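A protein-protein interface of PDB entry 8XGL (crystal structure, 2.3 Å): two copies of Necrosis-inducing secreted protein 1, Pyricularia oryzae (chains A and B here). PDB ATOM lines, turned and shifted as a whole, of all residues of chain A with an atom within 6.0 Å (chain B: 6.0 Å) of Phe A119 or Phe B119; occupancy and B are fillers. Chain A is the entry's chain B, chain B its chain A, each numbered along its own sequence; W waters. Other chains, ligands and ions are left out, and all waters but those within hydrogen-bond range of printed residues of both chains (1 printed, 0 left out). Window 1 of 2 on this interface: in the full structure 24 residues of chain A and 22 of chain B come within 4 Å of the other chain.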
ATOM      1  N   PHE A  42       4.762  21.632  -4.404  1.00  0.00           N
ATOM      2  CA  PHE A  42       6.013  20.900  -4.250  1.00  0.00           C
ATOM      3  C   PHE A  42       6.107  19.695  -5.182  1.00  0.00           C
ATOM      4  O   PHE A  42       7.173  19.441  -5.752  1.00  0.00           O
ATOM      5  CB  PHE A  42       6.180  20.462  -2.794  1.00  0.00           C
ATOM      6  CG  PHE A  42       6.299  21.611  -1.832  1.00  0.00           C
ATOM      7  CD1 PHE A  42       7.270  22.586  -2.014  1.00  0.00           C
ATOM      8  CD2 PHE A  42       5.440  21.723  -0.753  1.00  0.00           C
ATOM      9  CE1 PHE A  42       7.380  23.646  -1.137  1.00  0.00           C
ATOM     10  CE2 PHE A  42       5.546  22.783   0.127  1.00  0.00           C
ATOM     11  CZ  PHE A  42       6.521  23.746  -0.067  1.00  0.00           C
ATOM     12  N   GLY A  43       5.020  18.956  -5.358  1.00  0.00           N
ATOM     13  CA  GLY A  43       5.058  17.755  -6.171  1.00  0.00           C
ATOM     14  C   GLY A  43       3.679  17.143  -6.242  1.00  0.00           C
ATOM     15  O   GLY A  43       2.773  17.503  -5.483  1.00  0.00           O
ATOM     16  N   VAL A  45       1.852  13.317  -6.409  1.00  0.00           N
ATOM     17  CA  VAL A  45       1.848  11.860  -6.373  1.00  0.00           C
ATOM     18  C   VAL A  45       0.676  11.365  -7.209  1.00  0.00           C
ATOM     19  O   VAL A  45      -0.440  11.890  -7.108  1.00  0.00           O
ATOM     20  CB  VAL A  45       1.766  11.332  -4.929  1.00  0.00           C
ATOM     21  CG1 VAL A  45       0.477  11.765  -4.246  1.00  0.00           C
ATOM     22  CG2 VAL A  45       1.877   9.811  -4.921  1.00  0.00           C
ATOM     23  N   GLY A 106      -2.262  13.650  -6.067  1.00  0.00           N
ATOM     24  CA  GLY A 106      -2.109  14.292  -4.780  1.00  0.00           C
ATOM     25  C   GLY A 106      -1.042  15.361  -4.833  1.00  0.00           C
ATOM     26  O   GLY A 106       0.154  15.053  -4.897  1.00  0.00           O
ATOM     27  N   ALA A 107      -1.464  16.620  -4.816  1.00  0.00           N
ATOM     28  CA  ALA A 107      -0.562  17.760  -4.937  1.00  0.00           C
ATOM     29  C   ALA A 107      -0.258  18.316  -3.551  1.00  0.00           C
ATOM     30  O   ALA A 107      -1.153  18.826  -2.869  1.00  0.00           O
ATOM     31  CB  ALA A 107      -1.172  18.841  -5.826  1.00  0.00           C
ATOM     32  N   SER A 108       1.003  18.214  -3.145  1.00  0.00           N
ATOM     33  CA  SER A 108       1.463  18.809  -1.902  1.00  0.00           C
ATOM     34  C   SER A 108       1.738  20.293  -2.111  1.00  0.00           C
ATOM     35  O   SER A 108       2.153  20.721  -3.191  1.00  0.00           O
ATOM     36  CB  SER A 108       2.727  18.107  -1.420  1.00  0.00           C
ATOM     37  OG  SER A 108       3.716  18.154  -2.432  1.00  0.00           O
ATOM     38  N   TYR A 109       1.513  21.079  -1.063  1.00  0.00           N
ATOM     39  CA  TYR A 109       1.576  22.525  -1.201  1.00  0.00           C
ATOM     40  C   TYR A 109       1.976  23.171   0.119  1.00  0.00           C
ATOM     41  O   TYR A 109       1.940  22.552   1.186  1.00  0.00           O
ATOM     42  CB  TYR A 109       0.228  23.088  -1.667  1.00  0.00           C
ATOM     43  CG  TYR A 109      -0.875  22.885  -0.654  1.00  0.00           C
ATOM     44  CD1 TYR A 109      -1.004  23.731   0.442  1.00  0.00           C
ATOM     45  CD2 TYR A 109      -1.776  21.837  -0.780  1.00  0.00           C
ATOM     46  CE1 TYR A 109      -2.002  23.542   1.377  1.00  0.00           C
ATOM     47  CE2 TYR A 109      -2.777  21.640   0.151  1.00  0.00           C
ATOM     48  CZ  TYR A 109      -2.887  22.495   1.227  1.00  0.00           C
ATOM     49  OH  TYR A 109      -3.885  22.304   2.155  1.00  0.00           O
ATOM     50  N   THR A 117       0.749  23.743   5.121  1.00  0.00           N
ATOM     51  CA  THR A 117       1.131  22.668   4.219  1.00  0.00           C
ATOM     52  C   THR A 117       0.046  21.597   4.198  1.00  0.00           C
ATOM     53  O   THR A 117      -0.684  21.411   5.176  1.00  0.00           O
ATOM     54  CB  THR A 117       2.469  22.038   4.630  1.00  0.00           C
ATOM     55  OG1 THR A 117       2.341  21.433   5.921  1.00  0.00           O
ATOM     56  CG2 THR A 117       3.586  23.084   4.668  1.00  0.00           C
ATOM     57  N   GLY A 118      -0.054  20.897   3.075  1.00  0.00           N
ATOM     58  CA  GLY A 118      -1.028  19.829   2.960  1.00  0.00           C
ATOM     59  C   GLY A 118      -1.034  19.226   1.574  1.00  0.00           C
ATOM     60  O   GLY A 118      -0.094  19.402   0.795  1.00  0.00           O
ATOM     61  N   PHE A 119      -2.119  18.506   1.279  1.00  0.00           N
ATOM     62  CA  PHE A 119      -2.331  17.857  -0.005  1.00  0.00           C
ATOM     63  C   PHE A 119      -3.695  18.243  -0.554  1.00  0.00           C
ATOM     64  O   PHE A 119      -4.678  18.291   0.189  1.00  0.00           O
ATOM     65  CB  PHE A 119      -2.273  16.330   0.117  1.00  0.00           C
ATOM     66  CG  PHE A 119      -0.902  15.749  -0.049  1.00  0.00           C
ATOM     67  CD1 PHE A 119      -0.073  15.586   1.044  1.00  0.00           C
ATOM     68  CD2 PHE A 119      -0.453  15.332  -1.292  1.00  0.00           C
ATOM     69  CE1 PHE A 119       1.186  15.038   0.902  1.00  0.00           C
ATOM     70  CE2 PHE A 119       0.806  14.782  -1.440  1.00  0.00           C
ATOM     71  CZ  PHE A 119       1.627  14.634  -0.342  1.00  0.00           C
ATOM     72  N   ASN A 120      -3.752  18.516  -1.853  1.00  0.00           N
ATOM     73  CA  ASN A 120      -5.007  18.609  -2.582  1.00  0.00           C
ATOM     74  C   ASN A 120      -5.130  17.404  -3.503  1.00  0.00           C
ATOM     75  O   ASN A 120      -4.136  16.925  -4.058  1.00  0.00           O
ATOM     76  CB  ASN A 120      -5.091  19.897  -3.396  1.00  0.00           C
ATOM     77  CG  ASN A 120      -5.138  21.130  -2.524  1.00  0.00           C
ATOM     78  OD1 ASN A 120      -5.941  21.220  -1.591  1.00  0.00           O
ATOM     79  ND2 ASN A 120      -4.265  22.086  -2.813  1.00  0.00           N
ATOM     80  N   TYR A 121      -6.351  16.908  -3.650  1.00  0.00           N
ATOM     81  CA  TYR A 121      -6.604  15.676  -4.376  1.00  0.00           C
ATOM     82  C   TYR A 121      -7.514  15.960  -5.559  1.00  0.00           C
ATOM     83  O   TYR A 121      -8.511  16.676  -5.430  1.00  0.00           O
ATOM     84  CB  TYR A 121      -7.206  14.618  -3.447  1.00  0.00           C
ATOM     85  CG  TYR A 121      -6.284  14.295  -2.296  1.00  0.00           C
ATOM     86  CD1 TYR A 121      -5.158  13.509  -2.491  1.00  0.00           C
ATOM     87  CD2 TYR A 121      -6.518  14.803  -1.026  1.00  0.00           C
ATOM     88  CE1 TYR A 121      -4.298  13.222  -1.451  1.00  0.00           C
ATOM     89  CE2 TYR A 121      -5.664  14.517   0.024  1.00  0.00           C
ATOM     90  CZ  TYR A 121      -4.557  13.727  -0.194  1.00  0.00           C
ATOM     91  OH  TYR A 121      -3.701  13.440   0.845  1.00  0.00           O
ATOM     92  N   PHE B  42       8.569  11.809   0.005  1.00  0.00           N
ATOM     93  CA  PHE B  42       8.622  12.585  -1.231  1.00  0.00           C
ATOM     94  C   PHE B  42       9.530  13.800  -1.103  1.00  0.00           C
ATOM     95  O   PHE B  42      10.353  14.063  -1.986  1.00  0.00           O
ATOM     96  CB  PHE B  42       7.215  13.019  -1.640  1.00  0.00           C
ATOM     97  CG  PHE B  42       6.316  11.874  -1.969  1.00  0.00           C
ATOM     98  CD1 PHE B  42       6.670  10.975  -2.958  1.00  0.00           C
ATOM     99  CD2 PHE B  42       5.132  11.677  -1.280  1.00  0.00           C
ATOM    100  CE1 PHE B  42       5.857   9.911  -3.268  1.00  0.00           C
ATOM    101  CE2 PHE B  42       4.313  10.613  -1.584  1.00  0.00           C
ATOM    102  CZ  PHE B  42       4.677   9.725  -2.581  1.00  0.00           C
ATOM    103  N   GLY B  43       9.391  14.542  -0.017  1.00  0.00           N
ATOM    104  CA  GLY B  43      10.223  15.710   0.192  1.00  0.00           C
ATOM    105  C   GLY B  43       9.962  16.282   1.563  1.00  0.00           C
ATOM    106  O   GLY B  43       9.055  15.849   2.282  1.00  0.00           O
ATOM    107  N   VAL B  45       9.574  20.073   3.429  1.00  0.00           N
ATOM    108  CA  VAL B  45       9.474  21.527   3.451  1.00  0.00           C
ATOM    109  C   VAL B  45      10.052  22.018   4.767  1.00  0.00           C
ATOM    110  O   VAL B  45       9.781  21.450   5.832  1.00  0.00           O
ATOM    111  CB  VAL B  45       8.017  21.992   3.269  1.00  0.00           C
ATOM    112  CG1 VAL B  45       7.140  21.459   4.382  1.00  0.00           C
ATOM    113  CG2 VAL B  45       7.941  23.510   3.244  1.00  0.00           C
ATOM    114  N   GLY B 106       8.544  19.555   7.432  1.00  0.00           N
ATOM    115  CA  GLY B 106       7.317  18.908   7.026  1.00  0.00           C
ATOM    116  C   GLY B 106       7.604  17.861   5.976  1.00  0.00           C
ATOM    117  O   GLY B 106       7.891  18.193   4.821  1.00  0.00           O
ATOM    118  N   ALA B 107       7.542  16.591   6.370  1.00  0.00           N
ATOM    119  CA  ALA B 107       7.876  15.484   5.487  1.00  0.00           C
ATOM    120  C   ALA B 107       6.605  14.932   4.852  1.00  0.00           C
ATOM    121  O   ALA B 107       5.744  14.382   5.547  1.00  0.00           O
ATOM    122  CB  ALA B 107       8.610  14.385   6.252  1.00  0.00           C
ATOM    123  N   SER B 108       6.500  15.065   3.534  1.00  0.00           N
ATOM    124  CA  SER B 108       5.389  14.480   2.803  1.00  0.00           C
ATOM    125  C   SER B 108       5.660  13.000   2.562  1.00  0.00           C
ATOM    126  O   SER B 108       6.799  12.594   2.314  1.00  0.00           O
ATOM    127  CB  SER B 108       5.198  15.202   1.472  1.00  0.00           C
ATOM    128  OG  SER B 108       6.382  15.116   0.704  1.00  0.00           O
ATOM    129  N   TYR B 109       4.606  12.190   2.622  1.00  0.00           N
ATOM    130  CA  TYR B 109       4.796  10.751   2.555  1.00  0.00           C
ATOM    131  C   TYR B 109       3.606  10.080   1.885  1.00  0.00           C
ATOM    132  O   TYR B 109       2.517  10.651   1.773  1.00  0.00           O
ATOM    133  CB  TYR B 109       5.001  10.167   3.956  1.00  0.00           C
ATOM    134  CG  TYR B 109       3.778  10.319   4.822  1.00  0.00           C
ATOM    135  CD1 TYR B 109       2.724   9.416   4.738  1.00  0.00           C
ATOM    136  CD2 TYR B 109       3.664  11.378   5.711  1.00  0.00           C
ATOM    137  CE1 TYR B 109       1.600   9.560   5.519  1.00  0.00           C
ATOM    138  CE2 TYR B 109       2.545  11.530   6.500  1.00  0.00           C
ATOM    139  CZ  TYR B 109       1.515  10.618   6.400  1.00  0.00           C
ATOM    140  OH  TYR B 109       0.393  10.761   7.180  1.00  0.00           O
ATOM    141  N   THR B 117      -1.571   9.434   2.051  1.00  0.00           N
ATOM    142  CA  THR B 117      -0.597  10.501   1.889  1.00  0.00           C
ATOM    143  C   THR B 117      -0.856  11.596   2.914  1.00  0.00           C
ATOM    144  O   THR B 117      -1.990  11.802   3.358  1.00  0.00           O
ATOM    145  CB  THR B 117      -0.633  11.108   0.478  1.00  0.00           C
ATOM    146  OG1 THR B 117      -1.926  11.669   0.226  1.00  0.00           O
ATOM    147  CG2 THR B 117      -0.317  10.058  -0.580  1.00  0.00           C
ATOM    148  N   GLY B 118       0.208  12.295   3.285  1.00  0.00           N
ATOM    149  CA  GLY B 118       0.089  13.351   4.266  1.00  0.00           C
ATOM    150  C   GLY B 118       1.441  13.941   4.587  1.00  0.00           C
ATOM    151  O   GLY B 118       2.416  13.748   3.857  1.00  0.00           O
ATOM    152  N   PHE B 119       1.479  14.673   5.695  1.00  0.00           N
ATOM    153  CA  PHE B 119       2.694  15.294   6.198  1.00  0.00           C
ATOM    154  C   PHE B 119       2.936  14.841   7.630  1.00  0.00           C
ATOM    155  O   PHE B 119       2.004  14.803   8.438  1.00  0.00           O
ATOM    156  CB  PHE B 119       2.592  16.824   6.162  1.00  0.00           C
ATOM    157  CG  PHE B 119       2.970  17.437   4.844  1.00  0.00           C
ATOM    158  CD1 PHE B 119       2.029  17.582   3.840  1.00  0.00           C
ATOM    159  CD2 PHE B 119       4.262  17.890   4.615  1.00  0.00           C
ATOM    160  CE1 PHE B 119       2.369  18.150   2.633  1.00  0.00           C
ATOM    161  CE2 PHE B 119       4.606  18.461   3.408  1.00  0.00           C
ATOM    162  CZ  PHE B 119       3.658  18.594   2.416  1.00  0.00           C
ATOM    163  N   ASN B 120       4.181  14.484   7.933  1.00  0.00           N
ATOM    164  CA  ASN B 120       4.656  14.385   9.305  1.00  0.00           C
ATOM    165  C   ASN B 120       5.498  15.610   9.624  1.00  0.00           C
ATOM    166  O   ASN B 120       6.287  16.066   8.791  1.00  0.00           O
ATOM    167  CB  ASN B 120       5.492  13.128   9.520  1.00  0.00           C
ATOM    168  CG  ASN B 120       4.656  11.873   9.537  1.00  0.00           C
ATOM    169  OD1 ASN B 120       3.625  11.802  10.207  1.00  0.00           O
ATOM    170  ND2 ASN B 120       5.090  10.872   8.782  1.00  0.00           N
ATOM    171  N   TYR B 121       5.337  16.134  10.831  1.00  0.00           N
ATOM    172  CA  TYR B 121       6.015  17.350  11.245  1.00  0.00           C
ATOM    173  C   TYR B 121       6.997  17.051  12.371  1.00  0.00           C
ATOM    174  O   TYR B 121       6.716  16.244  13.262  1.00  0.00           O
ATOM    175  CB  TYR B 121       4.991  18.407  11.664  1.00  0.00           C
ATOM    176  CG  TYR B 121       4.012  18.715  10.549  1.00  0.00           C
ATOM    177  CD1 TYR B 121       4.381  19.520   9.477  1.00  0.00           C
ATOM    178  CD2 TYR B 121       2.731  18.171  10.546  1.00  0.00           C
ATOM    179  CE1 TYR B 121       3.497  19.792   8.444  1.00  0.00           C
ATOM    180  CE2 TYR B 121       1.840  18.440   9.517  1.00  0.00           C
ATOM    181  CZ  TYR B 121       2.228  19.249   8.470  1.00  0.00           C
ATOM    182  OH  TYR B 121       1.341  19.513   7.451  1.00  0.00           O
HETATM  183  O   HOH W   1      -4.248  14.311   3.673  1.00  0.00           O
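The side-chain hydroxyl of Tyr A121 sits at hydrogen-bond distance from the side-chain hydroxyl of Thr B117 (2.6 Å).
OG1 of Thr A117 is in hydrogen-bond range of OH of Tyr B121 (2.7 Å).
The backbone NH (N) of Phe B42 sits at hydrogen-bond distance from the backbone carbonyl oxygen (O) of Ser B108, 3.0 Å away.
O of Val B45 is in hydrogen-bond range of N of Gly B106 (2.8 Å).
The backbone NH of Tyr B109 is in hydrogen-bond range of the backbone carbonyl oxygen of Gly B118, 3.0 Å away.
O of Gly A43 is in hydrogen-bond range of N of Ser A108, 3.0 Å away.
The backbone carbonyl oxygen (O) of Val A45 sits at hydrogen-bond distance from the backbone NH (N) of Gly A106 (2.7 Å).
The backbone NH (N) of Tyr A109 lies within hydrogen-bond range of the backbone carbonyl oxygen (O) of Gly A118, at 3.0 Å.
Among the printed residues, merely in contact across the chains: Gly A118 with Phe B119 (3.3 Å), Phe A119 with Gly B118 (3.5 Å), Phe A42 with Val B45 (3.6 Å), Val A45 with Phe B42 (3.7 Å), Phe A119 with Phe B119 (3.8 Å), Thr A117 with Val B45 (3.9 Å) and Ser A108 with Phe B119 (3.98 Å).
Printed residues of chain B within 4 Å of Phe A42: Val B45.
Printed residues of chain B within 4 Å of Val A45: Phe B42.
Printed residues of chain B within 4 Å of Thr A117: Val B45 and Tyr B121.
Printed residues of chain A within 4 Å of Gly B118: Phe A119.
Phe B119 touches just these residues of chain A: Ser A108 (3.98 Å), Gly A118 (3.3 Å) and Phe A119 (3.8 Å).
Of the printed residues of chain A, Tyr B121 touches Thr A117 (2.7 Å).
The nearest residue of chain A that does not touch Phe B119 is Thr A117 (4.2 Å).
The nearest printed residue of chain B that does not touch Thr A117 is Phe B119 (4.2 Å).
Of the 12 printed residues of chain B, 6 touch a printed residue of chain A.
Hydrophobic or aromatic side chains of chain B within 4 Å of the printed part of chain A: Phe B42, Val B45, Phe B119 and Tyr B121.
Printed residues of chain A that touch a printed residue of chain B: Phe A42, Val A45, Ser A108, Thr A117, Gly A118, Phe A119 and Tyr A121.
Among the printed residues, 9 pairs touch across the chains.
Among the printed residues, no Asp or Glu carboxylate lies within 4 Å of a Lys or Arg side-chain nitrogen of the other chain.
Ser A108 touches Phe B119, but with the chains exchanged Phe A119 does not touch Ser B108 (4.05 Å).
Thr A117 touches Val B45, but with the chains exchanged Val A45 does not touch Thr B117 (4.1 Å).
Gly A118 touches Phe B119, and with the chains exchanged Phe A119 touches Gly B118.
Phe B119 touches its own counterpart, Phe A119.
Positions printed for both chains: 42, 43, 45, 106, 107, 108, 109, 117, 118, 119, 120 and 121.
Of the 9 pairs that touch across the chains among the printed residues, 7 have their exchanged pair printed and touching as well.
Water W1 bridges the side-chain hydroxyl (OH) of Tyr A121 (3.0 Å) and the backbone carbonyl oxygen (O) of Thr B117 (3.4 Å).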
